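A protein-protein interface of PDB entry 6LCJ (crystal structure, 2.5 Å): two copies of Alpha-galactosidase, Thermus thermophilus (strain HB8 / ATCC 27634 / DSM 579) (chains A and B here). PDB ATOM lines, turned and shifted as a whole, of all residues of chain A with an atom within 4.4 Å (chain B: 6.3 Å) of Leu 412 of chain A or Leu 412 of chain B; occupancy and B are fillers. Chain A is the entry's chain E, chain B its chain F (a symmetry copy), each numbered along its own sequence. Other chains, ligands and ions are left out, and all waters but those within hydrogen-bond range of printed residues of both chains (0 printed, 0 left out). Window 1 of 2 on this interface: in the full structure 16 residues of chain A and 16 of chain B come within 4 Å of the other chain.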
ATOM      1  N   PRO A 361      -7.965 -10.776  15.880  1.00  0.00           N
ATOM      2  CA  PRO A 361      -7.509  -9.955  17.007  1.00  0.00           C
ATOM      3  C   PRO A 361      -7.036 -10.794  18.199  1.00  0.00           C
ATOM      4  O   PRO A 361      -7.374 -10.519  19.349  1.00  0.00           O
ATOM      5  CB  PRO A 361      -8.744  -9.107  17.336  1.00  0.00           C
ATOM      6  CG  PRO A 361      -9.919  -9.837  16.770  1.00  0.00           C
ATOM      7  CD  PRO A 361      -9.429 -10.965  15.905  1.00  0.00           C
ATOM      8  N   TYR A 362      -6.268 -11.843  17.916  1.00  0.00           N
ATOM      9  CA  TYR A 362      -5.777 -12.744  18.952  1.00  0.00           C
ATOM     10  C   TYR A 362      -4.669 -13.605  18.369  1.00  0.00           C
ATOM     11  O   TYR A 362      -4.547 -13.759  17.148  1.00  0.00           O
ATOM     12  CB  TYR A 362      -6.886 -13.623  19.564  1.00  0.00           C
ATOM     13  CG  TYR A 362      -7.807 -14.321  18.598  1.00  0.00           C
ATOM     14  CD1 TYR A 362      -7.421 -15.497  17.950  1.00  0.00           C
ATOM     15  CD2 TYR A 362      -9.079 -13.823  18.349  1.00  0.00           C
ATOM     16  CE1 TYR A 362      -8.289 -16.143  17.065  1.00  0.00           C
ATOM     17  CE2 TYR A 362      -9.950 -14.461  17.481  1.00  0.00           C
ATOM     18  CZ  TYR A 362      -9.557 -15.616  16.838  1.00  0.00           C
ATOM     19  OH  TYR A 362     -10.439 -16.231  15.961  1.00  0.00           O
ATOM     20  N   PHE A 410     -10.728  -3.491  21.419  1.00  0.00           N
ATOM     21  CA  PHE A 410     -11.363  -4.526  20.607  1.00  0.00           C
ATOM     22  C   PHE A 410     -10.314  -5.384  19.911  1.00  0.00           C
ATOM     23  O   PHE A 410     -10.378  -5.631  18.705  1.00  0.00           O
ATOM     24  CB  PHE A 410     -12.332  -3.902  19.607  1.00  0.00           C
ATOM     25  CG  PHE A 410     -13.331  -3.005  20.259  1.00  0.00           C
ATOM     26  CD1 PHE A 410     -14.249  -3.525  21.172  1.00  0.00           C
ATOM     27  CD2 PHE A 410     -13.325  -1.638  20.011  1.00  0.00           C
ATOM     28  CE1 PHE A 410     -15.165  -2.707  21.806  1.00  0.00           C
ATOM     29  CE2 PHE A 410     -14.239  -0.806  20.643  1.00  0.00           C
ATOM     30  CZ  PHE A 410     -15.164  -1.343  21.540  1.00  0.00           C
ATOM     31  N   ASN A 411      -9.326  -5.823  20.694  1.00  0.00           N
ATOM     32  CA  ASN A 411      -8.183  -6.560  20.176  1.00  0.00           C
ATOM     33  C   ASN A 411      -7.505  -7.218  21.365  1.00  0.00           C
ATOM     34  O   ASN A 411      -7.348  -6.586  22.403  1.00  0.00           O
ATOM     35  CB  ASN A 411      -7.228  -5.622  19.415  1.00  0.00           C
ATOM     36  CG  ASN A 411      -6.067  -6.355  18.782  1.00  0.00           C
ATOM     37  OD1 ASN A 411      -6.020  -7.582  18.809  1.00  0.00           O
ATOM     38  ND2 ASN A 411      -5.104  -5.603  18.220  1.00  0.00           N
ATOM     39  N   LEU A 412      -7.156  -8.493  21.239  1.00  0.00           N
ATOM     40  CA  LEU A 412      -6.482  -9.197  22.321  1.00  0.00           C
ATOM     41  C   LEU A 412      -4.988  -9.300  22.099  1.00  0.00           C
ATOM     42  O   LEU A 412      -4.285  -9.825  22.966  1.00  0.00           O
ATOM     43  CB  LEU A 412      -7.042 -10.609  22.496  1.00  0.00           C
ATOM     44  CG  LEU A 412      -8.515 -10.772  22.832  1.00  0.00           C
ATOM     45  CD1 LEU A 412      -8.795 -12.252  23.126  1.00  0.00           C
ATOM     46  CD2 LEU A 412      -8.915  -9.846  23.993  1.00  0.00           C
ATOM     47  N   LEU A 413      -4.496  -8.820  20.962  1.00  0.00           N
ATOM     48  CA  LEU A 413      -3.100  -9.009  20.609  1.00  0.00           C
ATOM     49  C   LEU A 413      -2.192  -8.145  21.473  1.00  0.00           C
ATOM     50  O   LEU A 413      -2.532  -7.018  21.850  1.00  0.00           O
ATOM     51  CB  LEU A 413      -2.896  -8.672  19.141  1.00  0.00           C
ATOM     52  CG  LEU A 413      -3.420  -9.722  18.170  1.00  0.00           C
ATOM     53  CD1 LEU A 413      -3.421  -9.151  16.767  1.00  0.00           C
ATOM     54  CD2 LEU A 413      -2.557 -10.960  18.269  1.00  0.00           C
ATOM     55  N   SER A 414      -1.015  -8.666  21.763  1.00  0.00           N
ATOM     56  CA  SER A 414      -0.050  -7.867  22.498  1.00  0.00           C
ATOM     57  C   SER A 414       0.700  -6.927  21.558  1.00  0.00           C
ATOM     58  O   SER A 414       0.788  -7.167  20.352  1.00  0.00           O
ATOM     59  CB  SER A 414       0.936  -8.762  23.243  1.00  0.00           C
ATOM     60  OG  SER A 414       2.005  -9.142  22.401  1.00  0.00           O
ATOM     61  N   PRO B 361     -12.849 -12.370  27.610  1.00  0.00           N
ATOM     62  CA  PRO B 361     -13.000 -11.103  26.889  1.00  0.00           C
ATOM     63  C   PRO B 361     -13.538 -11.320  25.486  1.00  0.00           C
ATOM     64  O   PRO B 361     -13.055 -10.738  24.514  1.00  0.00           O
ATOM     65  CB  PRO B 361     -11.576 -10.540  26.883  1.00  0.00           C
ATOM     66  CG  PRO B 361     -10.705 -11.757  26.914  1.00  0.00           C
ATOM     67  CD  PRO B 361     -11.438 -12.797  27.686  1.00  0.00           C
ATOM     68  N   TYR B 362     -14.539 -12.182  25.374  1.00  0.00           N
ATOM     69  CA  TYR B 362     -15.167 -12.471  24.097  1.00  0.00           C
ATOM     70  C   TYR B 362     -16.489 -13.154  24.392  1.00  0.00           C
ATOM     71  O   TYR B 362     -16.679 -13.745  25.458  1.00  0.00           O
ATOM     72  CB  TYR B 362     -14.264 -13.329  23.183  1.00  0.00           C
ATOM     73  CG  TYR B 362     -13.658 -14.556  23.831  1.00  0.00           C
ATOM     74  CD1 TYR B 362     -14.401 -15.726  23.974  1.00  0.00           C
ATOM     75  CD2 TYR B 362     -12.334 -14.556  24.286  1.00  0.00           C
ATOM     76  CE1 TYR B 362     -13.855 -16.857  24.551  1.00  0.00           C
ATOM     77  CE2 TYR B 362     -11.774 -15.694  24.890  1.00  0.00           C
ATOM     78  CZ  TYR B 362     -12.540 -16.842  25.015  1.00  0.00           C
ATOM     79  OH  TYR B 362     -12.021 -17.977  25.611  1.00  0.00           O
ATOM     80  N   TRP B 363     -17.406 -13.056  23.435  1.00  0.00           N
ATOM     81  CA  TRP B 363     -18.751 -13.592  23.623  1.00  0.00           C
ATOM     82  C   TRP B 363     -18.748 -15.119  23.679  1.00  0.00           C
ATOM     83  O   TRP B 363     -19.265 -15.723  24.631  1.00  0.00           O
ATOM     84  CB  TRP B 363     -19.655 -13.087  22.496  1.00  0.00           C
ATOM     85  CG  TRP B 363     -21.059 -13.498  22.620  1.00  0.00           C
ATOM     86  CD1 TRP B 363     -21.741 -14.311  21.774  1.00  0.00           C
ATOM     87  CD2 TRP B 363     -21.980 -13.128  23.659  1.00  0.00           C
ATOM     88  NE1 TRP B 363     -23.030 -14.470  22.212  1.00  0.00           N
ATOM     89  CE2 TRP B 363     -23.207 -13.757  23.368  1.00  0.00           C
ATOM     90  CE3 TRP B 363     -21.888 -12.324  24.805  1.00  0.00           C
ATOM     91  CZ2 TRP B 363     -24.340 -13.615  24.184  1.00  0.00           C
ATOM     92  CZ3 TRP B 363     -23.020 -12.180  25.616  1.00  0.00           C
ATOM     93  CH2 TRP B 363     -24.224 -12.822  25.295  1.00  0.00           C
ATOM     94  N   ARG B 407     -13.206  -2.313  30.579  1.00  0.00           N
ATOM     95  CA  ARG B 407     -12.262  -1.908  29.557  1.00  0.00           C
ATOM     96  C   ARG B 407     -12.759  -2.305  28.169  1.00  0.00           C
ATOM     97  O   ARG B 407     -13.540  -3.241  28.006  1.00  0.00           O
ATOM     98  CB  ARG B 407     -10.900  -2.540  29.825  1.00  0.00           C
ATOM     99  CG  ARG B 407     -10.856  -4.008  29.540  1.00  0.00           C
ATOM    100  CD  ARG B 407      -9.644  -4.619  30.153  1.00  0.00           C
ATOM    101  NE  ARG B 407      -9.290  -5.898  29.556  1.00  0.00           N
ATOM    102  CZ  ARG B 407      -9.260  -7.054  30.214  1.00  0.00           C
ATOM    103  NH1 ARG B 407      -9.595  -7.105  31.504  1.00  0.00           N
ATOM    104  NH2 ARG B 407      -8.900  -8.162  29.575  1.00  0.00           N
ATOM    105  N   THR B 408     -12.310  -1.550  27.166  1.00  0.00           N
ATOM    106  CA  THR B 408     -12.367  -1.960  25.775  1.00  0.00           C
ATOM    107  C   THR B 408     -11.004  -2.335  25.214  1.00  0.00           C
ATOM    108  O   THR B 408     -10.935  -3.072  24.227  1.00  0.00           O
ATOM    109  CB  THR B 408     -12.964  -0.848  24.907  1.00  0.00           C
ATOM    110  OG1 THR B 408     -12.209   0.359  25.098  1.00  0.00           O
ATOM    111  CG2 THR B 408     -14.421  -0.622  25.273  1.00  0.00           C
ATOM    112  N   PHE B 410      -7.842  -4.643  25.100  1.00  0.00           N
ATOM    113  CA  PHE B 410      -7.586  -6.038  25.447  1.00  0.00           C
ATOM    114  C   PHE B 410      -8.881  -6.760  25.810  1.00  0.00           C
ATOM    115  O   PHE B 410      -8.982  -7.437  26.832  1.00  0.00           O
ATOM    116  CB  PHE B 410      -6.540  -6.124  26.564  1.00  0.00           C
ATOM    117  CG  PHE B 410      -5.273  -5.360  26.243  1.00  0.00           C
ATOM    118  CD1 PHE B 410      -4.541  -5.662  25.100  1.00  0.00           C
ATOM    119  CD2 PHE B 410      -4.837  -4.317  27.050  1.00  0.00           C
ATOM    120  CE1 PHE B 410      -3.366  -4.948  24.783  1.00  0.00           C
ATOM    121  CE2 PHE B 410      -3.673  -3.599  26.736  1.00  0.00           C
ATOM    122  CZ  PHE B 410      -2.935  -3.918  25.604  1.00  0.00           C
ATOM    123  N   ASN B 411      -9.878  -6.616  24.935  1.00  0.00           N
ATOM    124  CA  ASN B 411     -11.220  -7.138  25.166  1.00  0.00           C
ATOM    125  C   ASN B 411     -12.000  -7.102  23.857  1.00  0.00           C
ATOM    126  O   ASN B 411     -12.034  -6.059  23.208  1.00  0.00           O
ATOM    127  CB  ASN B 411     -11.929  -6.314  26.246  1.00  0.00           C
ATOM    128  CG  ASN B 411     -13.284  -6.871  26.616  1.00  0.00           C
ATOM    129  OD1 ASN B 411     -13.692  -7.923  26.128  1.00  0.00           O
ATOM    130  ND2 ASN B 411     -13.990  -6.170  27.492  1.00  0.00           N
ATOM    131  N   LEU B 412     -12.617  -8.215  23.446  1.00  0.00           N
ATOM    132  CA  LEU B 412     -13.424  -8.241  22.226  1.00  0.00           C
ATOM    133  C   LEU B 412     -14.906  -8.063  22.507  1.00  0.00           C
ATOM    134  O   LEU B 412     -15.704  -8.037  21.567  1.00  0.00           O
ATOM    135  CB  LEU B 412     -13.222  -9.548  21.442  1.00  0.00           C
ATOM    136  CG  LEU B 412     -11.786  -9.895  21.042  1.00  0.00           C
ATOM    137  CD1 LEU B 412     -11.699 -11.207  20.278  1.00  0.00           C
ATOM    138  CD2 LEU B 412     -11.086  -8.756  20.272  1.00  0.00           C
ATOM    139  N   LEU B 413     -15.292  -7.956  23.774  1.00  0.00           N
ATOM    140  CA  LEU B 413     -16.697  -7.812  24.109  1.00  0.00           C
ATOM    141  C   LEU B 413     -17.223  -6.480  23.605  1.00  0.00           C
ATOM    142  O   LEU B 413     -16.517  -5.466  23.637  1.00  0.00           O
ATOM    143  CB  LEU B 413     -16.896  -7.909  25.611  1.00  0.00           C
ATOM    144  CG  LEU B 413     -16.594  -9.256  26.226  1.00  0.00           C
ATOM    145  CD1 LEU B 413     -16.530  -9.086  27.719  1.00  0.00           C
ATOM    146  CD2 LEU B 413     -17.678 -10.225  25.834  1.00  0.00           C
ATOM    147  N   SER B 414     -18.461  -6.488  23.119  1.00  0.00           N
ATOM    148  CA  SER B 414     -19.099  -5.234  22.754  1.00  0.00           C
ATOM    149  C   SER B 414     -19.579  -4.521  24.015  1.00  0.00           C
ATOM    150  O   SER B 414     -19.781  -5.159  25.050  1.00  0.00           O
ATOM    151  CB  SER B 414     -20.282  -5.484  21.824  1.00  0.00           C
ATOM    152  OG  SER B 414     -21.399  -5.958  22.559  1.00  0.00           O
ATOM    153  N   GLU B 417     -22.755  -6.136  25.206  1.00  0.00           N
ATOM    154  CA  GLU B 417     -22.557  -7.389  25.927  1.00  0.00           C
ATOM    155  C   GLU B 417     -22.043  -7.130  27.338  1.00  0.00           C
ATOM    156  O   GLU B 417     -22.509  -7.746  28.303  1.00  0.00           O
ATOM    157  CB  GLU B 417     -21.608  -8.296  25.145  1.00  0.00           C
ATOM    158  CG  GLU B 417     -22.191  -8.802  23.811  1.00  0.00           C
ATOM    159  CD  GLU B 417     -21.121  -9.166  22.783  1.00  0.00           C
ATOM    160  OE1 GLU B 417     -19.953  -8.745  22.935  1.00  0.00           O
ATOM    161  OE2 GLU B 417     -21.439  -9.879  21.811  1.00  0.00           O
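Hydrophobic or aromatic side chains of chain B that line the printed part of chain A: Pro 361, Phe 410 and Leu 412.
Hydrophobic or aromatic side chains of chain A that line the printed part of chain B: Pro 361, Phe 410 and Leu 412.
Along chain A the printed residues that touch a printed residue of chain B span positions 361 to 413.
Among the printed residues, no Asp or Glu carboxylate lies within 4 Å of a Lys or Arg side-chain nitrogen of the other chain.
Pro 361 of chain A touches Leu 412 of chain B.
Leu 412 of chain B touches Phe 410 of chain A.
CE1 of Phe 410 of chain A touches O of Leu 413 of chain B, 3.6 Å away.
Asn 411 of chain A touches Asn 411 of chain B.
Asn 411 of chain A touches Leu 412 of chain B (N to CD2, 3.4 Å).
Leu 412 of chain A touches Pro 361 of chain B.
CD2 of Leu 412 of chain A touches C of Phe 410 of chain B, at 3.6 Å.
N of Asn 411 of chain B touches CD2 of Leu 412 of chain A, 3.5 Å away.
Leu 412 of chain B touches Leu 412 of chain A.
O of Leu 413 of chain A touches CE1 of Phe 410 of chain B, 3.7 Å away.
Phe 410 of chain A touches Asn 411 of chain B, and with the chains exchanged Asn 411 of chain A touches Phe 410 of chain B.
Phe 410 of chain A touches Leu 413 of chain B, and with the chains exchanged Leu 413 of chain A touches Phe 410 of chain B.
Asn 411 of chain B touches its own counterpart, Asn 411 of chain A.
Asn 411 of chain A touches Leu 412 of chain B, and with the chains exchanged Leu 412 of chain A touches Asn 411 of chain B.
Positions printed for both chains: 361, 362, 410, 411, 412, 413 and 414.
Of the 13 pairs that touch across the chains among the printed residues, 12 have their exchanged pair printed and touching as well.
Of chain B, only Pro 361, Phe 410, Asn 411 and Leu 412 come within 4 Å of Leu 412 of chain A.
Of chain A, only Pro 361, Phe 410, Asn 411 and Leu 412 come within 4 Å of Leu 412 of chain B.
Printed residues of chain A within 4 Å of Leu 413 of chain B: Phe 410.
Of the printed residues of chain A, Phe 410 of chain B touches Asn 411, Leu 412 and Leu 413.
Printed residues of chain A within 4 Å of Pro 361 of chain B: Leu 412 (3.9 Å).
Of the printed residues of chain B, Pro 361 of chain A touches Leu 412.
Printed residues of chain B within 4 Å of Phe 410 of chain A: Thr 408, Asn 411, Leu 412 and Leu 413.
The nearest residue of chain A that does not touch Leu 412 of chain B is Tyr 362 of chain A (4.2 Å).
The side-chain amide oxygen (OD1) of Asn 411 of chain A lies close to the backbone carbonyl oxygen (O) of Pro 361 of chain A (3.3 Å).
The backbone carbonyl oxygen of Pro 361 of chain A lies within hydrogen-bond range of the backbone NH of Leu 412 of chain A.
The backbone NH (N) of Leu 413 of chain A lies within hydrogen-bond range of the side-chain amide oxygen (OD1) of Asn 411 of chain A (2.9 Å).
The side-chain amide oxygen (OD1) of Asn 411 of chain B sits close to the backbone carbonyl oxygen (O) of Pro 361 of chain B (3.3 Å).
O of Phe 410 of chain B is in hydrogen-bond range of NH2 of Arg 407 of chain B (2.8 Å).
O of Arg 407 of chain B lies within hydrogen-bond range of ND2 of Asn 411 of chain B, at 3.0 Å.
The backbone carbonyl oxygen (O) of Thr 408 of chain B lies within hydrogen-bond range of the backbone NH (N) of Phe 410 of chain A, 2.8 Å away.
The backbone NH (N) of Phe 410 of chain A lies close to the backbone carbonyl oxygen (O) of Asn 411 of chain B, 3.4 Å away.
The backbone carbonyl oxygen (O) of Asn 411 of chain A lies close to the backbone NH (N) of Phe 410 of chain B (3.4 Å).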
